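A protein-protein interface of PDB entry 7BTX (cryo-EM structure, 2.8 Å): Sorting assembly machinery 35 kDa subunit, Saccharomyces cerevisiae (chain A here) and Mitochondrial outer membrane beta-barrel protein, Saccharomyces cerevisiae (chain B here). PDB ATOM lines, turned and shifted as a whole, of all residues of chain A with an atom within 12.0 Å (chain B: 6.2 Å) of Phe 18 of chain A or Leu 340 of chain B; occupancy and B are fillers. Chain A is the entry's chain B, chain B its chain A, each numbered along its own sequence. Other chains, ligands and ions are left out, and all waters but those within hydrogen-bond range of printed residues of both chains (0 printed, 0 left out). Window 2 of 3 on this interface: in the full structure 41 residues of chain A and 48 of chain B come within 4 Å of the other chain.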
ATOM      1  N   ASP A  16      30.378   6.170  -0.948  1.00  0.00           N
ATOM      2  CA  ASP A  16      29.007   5.816  -0.602  1.00  0.00           C
ATOM      3  C   ASP A  16      28.418   4.724  -1.497  1.00  0.00           C
ATOM      4  O   ASP A  16      27.217   4.696  -1.750  1.00  0.00           O
ATOM      5  CB  ASP A  16      28.123   7.082  -0.589  1.00  0.00           C
ATOM      6  CG  ASP A  16      28.122   7.857  -1.914  1.00  0.00           C
ATOM      7  OD1 ASP A  16      28.063   7.272  -3.016  1.00  0.00           O
ATOM      8  OD2 ASP A  16      28.189   9.104  -1.840  1.00  0.00           O
ATOM      9  N   THR A  17      29.279   3.838  -1.987  1.00  0.00           N
ATOM     10  CA  THR A  17      28.854   2.590  -2.597  1.00  0.00           C
ATOM     11  C   THR A  17      29.024   1.414  -1.649  1.00  0.00           C
ATOM     12  O   THR A  17      28.820   0.265  -2.050  1.00  0.00           O
ATOM     13  CB  THR A  17      29.632   2.336  -3.888  1.00  0.00           C
ATOM     14  OG1 THR A  17      29.103   1.180  -4.548  1.00  0.00           O
ATOM     15  CG2 THR A  17      31.108   2.117  -3.591  1.00  0.00           C
ATOM     16  N   PHE A  18      29.371   1.685  -0.395  1.00  0.00           N
ATOM     17  CA  PHE A  18      29.808   0.674   0.562  1.00  0.00           C
ATOM     18  C   PHE A  18      28.769  -0.282   1.140  1.00  0.00           C
ATOM     19  O   PHE A  18      29.125  -1.442   1.387  1.00  0.00           O
ATOM     20  CB  PHE A  18      30.737   1.237   1.634  1.00  0.00           C
ATOM     21  CG  PHE A  18      32.133   1.443   1.146  1.00  0.00           C
ATOM     22  CD1 PHE A  18      32.985   0.359   1.010  1.00  0.00           C
ATOM     23  CD2 PHE A  18      32.593   2.706   0.810  1.00  0.00           C
ATOM     24  CE1 PHE A  18      34.272   0.528   0.560  1.00  0.00           C
ATOM     25  CE2 PHE A  18      33.885   2.885   0.362  1.00  0.00           C
ATOM     26  CZ  PHE A  18      34.727   1.793   0.236  1.00  0.00           C
ATOM     27  N   PRO A  19      27.517   0.110   1.394  1.00  0.00           N
ATOM     28  CA  PRO A  19      26.518  -0.936   1.656  1.00  0.00           C
ATOM     29  C   PRO A  19      26.252  -1.701   0.370  1.00  0.00           C
ATOM     30  O   PRO A  19      25.536  -1.234  -0.514  1.00  0.00           O
ATOM     31  CB  PRO A  19      25.288  -0.151   2.124  1.00  0.00           C
ATOM     32  CG  PRO A  19      25.837   1.078   2.688  1.00  0.00           C
ATOM     33  CD  PRO A  19      27.022   1.427   1.835  1.00  0.00           C
ATOM     34  N   LEU A  20      26.847  -2.889   0.278  1.00  0.00           N
ATOM     35  CA  LEU A  20      26.791  -3.664  -0.951  1.00  0.00           C
ATOM     36  C   LEU A  20      25.453  -4.353  -1.117  1.00  0.00           C
ATOM     37  O   LEU A  20      25.053  -4.647  -2.248  1.00  0.00           O
ATOM     38  CB  LEU A  20      27.926  -4.687  -0.971  1.00  0.00           C
ATOM     39  CG  LEU A  20      29.307  -4.154  -0.573  1.00  0.00           C
ATOM     40  CD1 LEU A  20      30.267  -5.290  -0.312  1.00  0.00           C
ATOM     41  CD2 LEU A  20      29.858  -3.229  -1.639  1.00  0.00           C
ATOM     42  N   GLN A  21      24.761  -4.619  -0.017  1.00  0.00           N
ATOM     43  CA  GLN A  21      23.384  -5.078  -0.041  1.00  0.00           C
ATOM     44  C   GLN A  21      22.607  -4.334   1.028  1.00  0.00           C
ATOM     45  O   GLN A  21      23.068  -4.204   2.163  1.00  0.00           O
ATOM     46  CB  GLN A  21      23.282  -6.584   0.197  1.00  0.00           C
ATOM     47  CG  GLN A  21      23.461  -7.416  -1.044  1.00  0.00           C
ATOM     48  CD  GLN A  21      23.254  -8.886  -0.781  1.00  0.00           C
ATOM     49  OE1 GLN A  21      23.165  -9.315   0.368  1.00  0.00           O
ATOM     50  NE2 GLN A  21      23.166  -9.672  -1.847  1.00  0.00           N
ATOM     51  N   THR A  22      21.440  -3.829   0.655  1.00  0.00           N
ATOM     52  CA  THR A  22      20.484  -3.291   1.603  1.00  0.00           C
ATOM     53  C   THR A  22      19.183  -4.058   1.459  1.00  0.00           C
ATOM     54  O   THR A  22      18.782  -4.410   0.347  1.00  0.00           O
ATOM     55  CB  THR A  22      20.243  -1.795   1.403  1.00  0.00           C
ATOM     56  OG1 THR A  22      19.792  -1.554   0.066  1.00  0.00           O
ATOM     57  CG2 THR A  22      21.514  -1.006   1.667  1.00  0.00           C
ATOM     58  N   TYR A  23      18.540  -4.330   2.584  1.00  0.00           N
ATOM     59  CA  TYR A  23      17.321  -5.116   2.621  1.00  0.00           C
ATOM     60  C   TYR A  23      16.138  -4.225   2.972  1.00  0.00           C
ATOM     61  O   TYR A  23      16.295  -3.057   3.329  1.00  0.00           O
ATOM     62  CB  TYR A  23      17.453  -6.260   3.629  1.00  0.00           C
ATOM     63  CG  TYR A  23      18.804  -6.932   3.620  1.00  0.00           C
ATOM     64  CD1 TYR A  23      19.152  -7.823   2.613  1.00  0.00           C
ATOM     65  CD2 TYR A  23      19.728  -6.684   4.620  1.00  0.00           C
ATOM     66  CE1 TYR A  23      20.383  -8.441   2.605  1.00  0.00           C
ATOM     67  CE2 TYR A  23      20.961  -7.294   4.615  1.00  0.00           C
ATOM     68  CZ  TYR A  23      21.281  -8.171   3.606  1.00  0.00           C
ATOM     69  OH  TYR A  23      22.507  -8.783   3.604  1.00  0.00           O
ATOM     70  N   ARG B 245      30.243  -2.526  15.523  1.00  0.00           N
ATOM     71  CA  ARG B 245      30.789  -1.218  15.204  1.00  0.00           C
ATOM     72  C   ARG B 245      30.400  -0.809  13.798  1.00  0.00           C
ATOM     73  O   ARG B 245      30.164  -1.645  12.926  1.00  0.00           O
ATOM     74  CB  ARG B 245      32.312  -1.217  15.316  1.00  0.00           C
ATOM     75  CG  ARG B 245      32.873  -1.689  16.623  1.00  0.00           C
ATOM     76  CD  ARG B 245      34.364  -1.920  16.485  1.00  0.00           C
ATOM     77  NE  ARG B 245      34.953  -2.555  17.655  1.00  0.00           N
ATOM     78  CZ  ARG B 245      34.953  -3.862  17.872  1.00  0.00           C
ATOM     79  NH1 ARG B 245      35.511  -4.353  18.963  1.00  0.00           N
ATOM     80  NH2 ARG B 245      34.393  -4.681  17.000  1.00  0.00           N
ATOM     81  N   GLY B 246      30.361   0.495  13.575  1.00  0.00           N
ATOM     82  CA  GLY B 246      29.929   1.048  12.319  1.00  0.00           C
ATOM     83  C   GLY B 246      28.444   1.186  12.212  1.00  0.00           C
ATOM     84  O   GLY B 246      27.922   1.293  11.106  1.00  0.00           O
ATOM     85  N   PHE B 292      38.727  -5.311  12.176  1.00  0.00           N
ATOM     86  CA  PHE B 292      37.594  -6.060  12.692  1.00  0.00           C
ATOM     87  C   PHE B 292      36.595  -6.360  11.589  1.00  0.00           C
ATOM     88  O   PHE B 292      36.525  -5.670  10.575  1.00  0.00           O
ATOM     89  CB  PHE B 292      36.888  -5.333  13.849  1.00  0.00           C
ATOM     90  CG  PHE B 292      36.328  -3.985  13.495  1.00  0.00           C
ATOM     91  CD1 PHE B 292      37.107  -2.853  13.624  1.00  0.00           C
ATOM     92  CD2 PHE B 292      35.014  -3.840  13.086  1.00  0.00           C
ATOM     93  CE1 PHE B 292      36.608  -1.621  13.317  1.00  0.00           C
ATOM     94  CE2 PHE B 292      34.518  -2.615  12.777  1.00  0.00           C
ATOM     95  CZ  PHE B 292      35.315  -1.505  12.901  1.00  0.00           C
ATOM     96  N   THR B 319      26.158  -6.292   8.670  1.00  0.00           N
ATOM     97  CA  THR B 319      27.580  -6.510   8.867  1.00  0.00           C
ATOM     98  C   THR B 319      28.362  -5.234   8.595  1.00  0.00           C
ATOM     99  O   THR B 319      27.871  -4.305   7.953  1.00  0.00           O
ATOM    100  CB  THR B 319      28.075  -7.643   7.966  1.00  0.00           C
ATOM    101  OG1 THR B 319      27.493  -7.501   6.670  1.00  0.00           O
ATOM    102  CG2 THR B 319      27.646  -8.974   8.531  1.00  0.00           C
ATOM    103  N   SER B 320      29.590  -5.196   9.111  1.00  0.00           N
ATOM    104  CA  SER B 320      30.482  -4.062   8.921  1.00  0.00           C
ATOM    105  C   SER B 320      31.912  -4.507   9.169  1.00  0.00           C
ATOM    106  O   SER B 320      32.165  -5.395   9.982  1.00  0.00           O
ATOM    107  CB  SER B 320      30.132  -2.902   9.852  1.00  0.00           C
ATOM    108  OG  SER B 320      30.556  -3.161  11.176  1.00  0.00           O
ATOM    109  N   THR B 321      32.844  -3.876   8.464  1.00  0.00           N
ATOM    110  CA  THR B 321      34.267  -4.107   8.663  1.00  0.00           C
ATOM    111  C   THR B 321      34.976  -2.769   8.786  1.00  0.00           C
ATOM    112  O   THR B 321      34.444  -1.731   8.396  1.00  0.00           O
ATOM    113  CB  THR B 321      34.881  -4.922   7.520  1.00  0.00           C
ATOM    114  OG1 THR B 321      36.278  -5.109   7.765  1.00  0.00           O
ATOM    115  CG2 THR B 321      34.700  -4.209   6.204  1.00  0.00           C
ATOM    116  N   GLY B 322      36.179  -2.788   9.330  1.00  0.00           N
ATOM    117  CA  GLY B 322      36.903  -1.548   9.486  1.00  0.00           C
ATOM    118  C   GLY B 322      38.272  -1.758  10.091  1.00  0.00           C
ATOM    119  O   GLY B 322      38.556  -2.786  10.709  1.00  0.00           O
ATOM    120  N   PHE B 338      38.076   3.383  11.640  1.00  0.00           N
ATOM    121  CA  PHE B 338      37.462   3.833  10.397  1.00  0.00           C
ATOM    122  C   PHE B 338      36.669   2.657   9.850  1.00  0.00           C
ATOM    123  O   PHE B 338      37.256   1.667   9.412  1.00  0.00           O
ATOM    124  CB  PHE B 338      38.510   4.304   9.392  1.00  0.00           C
ATOM    125  CG  PHE B 338      37.926   4.912   8.146  1.00  0.00           C
ATOM    126  CD1 PHE B 338      37.594   6.252   8.113  1.00  0.00           C
ATOM    127  CD2 PHE B 338      37.714   4.147   7.011  1.00  0.00           C
ATOM    128  CE1 PHE B 338      37.057   6.815   6.979  1.00  0.00           C
ATOM    129  CE2 PHE B 338      37.174   4.706   5.878  1.00  0.00           C
ATOM    130  CZ  PHE B 338      36.848   6.040   5.863  1.00  0.00           C
ATOM    131  N   THR B 339      35.346   2.768   9.853  1.00  0.00           N
ATOM    132  CA  THR B 339      34.484   1.625   9.610  1.00  0.00           C
ATOM    133  C   THR B 339      33.668   1.837   8.340  1.00  0.00           C
ATOM    134  O   THR B 339      33.260   2.954   8.024  1.00  0.00           O
ATOM    135  CB  THR B 339      33.543   1.396  10.804  1.00  0.00           C
ATOM    136  OG1 THR B 339      34.285   1.489  12.022  1.00  0.00           O
ATOM    137  CG2 THR B 339      32.965   0.008  10.750  1.00  0.00           C
ATOM    138  N   LEU B 340      33.447   0.750   7.601  1.00  0.00           N
ATOM    139  CA  LEU B 340      32.499   0.721   6.503  1.00  0.00           C
ATOM    140  C   LEU B 340      31.451  -0.347   6.781  1.00  0.00           C
ATOM    141  O   LEU B 340      31.784  -1.413   7.304  1.00  0.00           O
ATOM    142  CB  LEU B 340      33.173   0.413   5.156  1.00  0.00           C
ATOM    143  CG  LEU B 340      33.966   1.499   4.427  1.00  0.00           C
ATOM    144  CD1 LEU B 340      33.170   2.793   4.354  1.00  0.00           C
ATOM    145  CD2 LEU B 340      35.353   1.709   5.005  1.00  0.00           C
ATOM    146  N   PRO B 341      30.186  -0.096   6.461  1.00  0.00           N
ATOM    147  CA  PRO B 341      29.180  -1.156   6.580  1.00  0.00           C
ATOM    148  C   PRO B 341      29.072  -2.002   5.324  1.00  0.00           C
ATOM    149  O   PRO B 341      28.895  -1.473   4.227  1.00  0.00           O
ATOM    150  CB  PRO B 341      27.887  -0.378   6.850  1.00  0.00           C
ATOM    151  CG  PRO B 341      28.110   0.943   6.243  1.00  0.00           C
ATOM    152  CD  PRO B 341      29.577   1.225   6.257  1.00  0.00           C
ATOM    153  N   ILE B 342      29.170  -3.319   5.465  1.00  0.00           N
ATOM    154  CA  ILE B 342      29.097  -4.197   4.303  1.00  0.00           C
ATOM    155  C   ILE B 342      27.654  -4.393   3.868  1.00  0.00           C
ATOM    156  O   ILE B 342      27.272  -4.040   2.748  1.00  0.00           O
ATOM    157  CB  ILE B 342      29.787  -5.538   4.599  1.00  0.00           C
ATOM    158  CG1 ILE B 342      31.272  -5.310   4.841  1.00  0.00           C
ATOM    159  CG2 ILE B 342      29.595  -6.502   3.449  1.00  0.00           C
ATOM    160  CD1 ILE B 342      31.955  -4.586   3.707  1.00  0.00           C
ATOM    161  N   THR B 343      26.831  -4.960   4.740  1.00  0.00           N
ATOM    162  CA  THR B 343      25.402  -5.078   4.512  1.00  0.00           C
ATOM    163  C   THR B 343      24.663  -4.427   5.668  1.00  0.00           C
ATOM    164  O   THR B 343      25.155  -4.393   6.797  1.00  0.00           O
ATOM    165  CB  THR B 343      24.963  -6.539   4.378  1.00  0.00           C
ATOM    166  OG1 THR B 343      25.410  -7.279   5.517  1.00  0.00           O
ATOM    167  CG2 THR B 343      25.550  -7.160   3.129  1.00  0.00           C
ATOM    168  N   ILE B 350      23.787   4.215  10.204  1.00  0.00           N
ATOM    169  CA  ILE B 350      24.763   3.427   9.462  1.00  0.00           C
ATOM    170  C   ILE B 350      26.202   3.884   9.665  1.00  0.00           C
ATOM    171  O   ILE B 350      27.114   3.160   9.246  1.00  0.00           O
ATOM    172  CB  ILE B 350      24.397   3.392   7.964  1.00  0.00           C
ATOM    173  CG1 ILE B 350      24.738   2.040   7.348  1.00  0.00           C
ATOM    174  CG2 ILE B 350      25.040   4.538   7.187  1.00  0.00           C
ATOM    175  CD1 ILE B 350      24.068   1.807   6.029  1.00  0.00           C
ATOM    176  N   ARG B 351      26.438   5.059  10.274  1.00  0.00           N
ATOM    177  CA  ARG B 351      27.727   5.564  10.782  1.00  0.00           C
ATOM    178  C   ARG B 351      28.973   5.315   9.925  1.00  0.00           C
ATOM    179  O   ARG B 351      29.893   4.608  10.350  1.00  0.00           O
ATOM    180  CB  ARG B 351      27.980   5.007  12.182  1.00  0.00           C
ATOM    181  CG  ARG B 351      28.838   5.904  13.072  1.00  0.00           C
ATOM    182  CD  ARG B 351      28.117   7.175  13.441  1.00  0.00           C
ATOM    183  NE  ARG B 351      28.939   8.055  14.259  1.00  0.00           N
ATOM    184  CZ  ARG B 351      28.486   9.154  14.853  1.00  0.00           C
ATOM    185  NH1 ARG B 351      27.214   9.500  14.721  1.00  0.00           N
ATOM    186  NH2 ARG B 351      29.302   9.904  15.582  1.00  0.00           N
ATOM    187  N   LYS B 352      29.006   5.848   8.708  1.00  0.00           N
ATOM    188  CA  LYS B 352      30.171   5.661   7.854  1.00  0.00           C
ATOM    189  C   LYS B 352      31.330   6.526   8.325  1.00  0.00           C
ATOM    190  O   LYS B 352      31.136   7.636   8.826  1.00  0.00           O
ATOM    191  CB  LYS B 352      29.833   5.994   6.404  1.00  0.00           C
ATOM    192  CG  LYS B 352      29.406   4.804   5.594  1.00  0.00           C
ATOM    193  CD  LYS B 352      29.156   5.159   4.148  1.00  0.00           C
ATOM    194  CE  LYS B 352      27.703   5.524   3.932  1.00  0.00           C
ATOM    195  NZ  LYS B 352      27.341   5.524   2.493  1.00  0.00           N
ATOM    196  N   GLY B 353      32.541   6.009   8.170  1.00  0.00           N
ATOM    197  CA  GLY B 353      33.719   6.790   8.470  1.00  0.00           C
ATOM    198  C   GLY B 353      34.313   6.513   9.830  1.00  0.00           C
ATOM    199  O   GLY B 353      34.429   5.358  10.241  1.00  0.00           O
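Among the printed residues, pairs that only touch across the chains: Pro 19 of chain A with Ile 342 of chain B (3.4 Å), Tyr 23 of chain A with Thr 343 of chain B (3.4 Å), Gln 21 of chain A with Thr 343 of chain B (3.4 Å), Pro 19 of chain A with Pro 341 of chain B (3.5 Å), Asp 16 of chain A with Lys 352 of chain B (3.5 Å), Phe 18 of chain A with Leu 340 of chain B (3.6 Å), Gln 21 of chain A with Ile 342 of chain B (3.8 Å) and Pro 19 of chain A with Ile 350 of chain B (3.9 Å).
The backbone carbonyl oxygen of Thr 319 of chain B is in hydrogen-bond range of the backbone NH of Ile 342 of chain B (3.0 Å). The backbone carbonyl oxygen of Thr 343 of chain B sits at hydrogen-bond distance from the backbone NH of Thr 319 of chain B, 2.8 Å away. The backbone carbonyl oxygen (O) of Thr 321 of chain B sits at hydrogen-bond distance from the backbone NH (N) of Leu 340 of chain B. The side-chain amide oxygen (OE1) of Gln 21 of chain A sits at hydrogen-bond distance from the side-chain hydroxyl (OH) of Tyr 23 of chain A (3.3 Å).
Hydrophobic or aromatic side chains of chain A within 4 Å of the printed part of chain B: Phe 18, Pro 19, Leu 20 and Tyr 23. Of the 17 printed residues of chain B, 6 touch a printed residue of chain A. Hydrophobic or aromatic side chains of chain B within 4 Å of the printed part of chain A: Leu 340 and Ile 350. Among the printed residues, no Asp or Glu carboxylate lies within 4 Å of a Lys or Arg side-chain nitrogen of the other chain.
Printed residues of chain B within 4 Å of Asp 16 of chain A: Lys 352. Of chain B, only Leu 340, Pro 341 and Ile 342 come within 4 Å of Phe 18 of chain A. Printed residues of chain B within 4 Å of Pro 19 of chain A: Pro 341 (3.5 Å), Ile 342 (3.4 Å) and Ile 350 (3.9 Å). Printed residues of chain B within 4 Å of Gln 21 of chain A: Ile 342 and Thr 343. Gly 246 of chain B touches none of the printed residues of chain A. No residue of chain A comes within 4 Å of Gly 322 of chain B. No residue of chain A comes within 4 Å of Phe 338 of chain B. Leu 340 of chain B touches just one residue of chain A: Phe 18 (3.6 Å). Pro 341 of chain B touches two residues of chain A. Printed residues of chain A within 4 Å of Thr 343 of chain B: Gln 21 (3.4 Å) and Tyr 23 (3.4 Å).
O of Ile 342 of chain B sits at hydrogen-bond distance from N of Leu 20 of chain A (2.8 Å). O of Phe 18 of chain A sits close to O of Pro 341 of chain B, at 2.8 Å. O of Phe 18 of chain A sits close to O of Ile 342 of chain B (3.5 Å).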
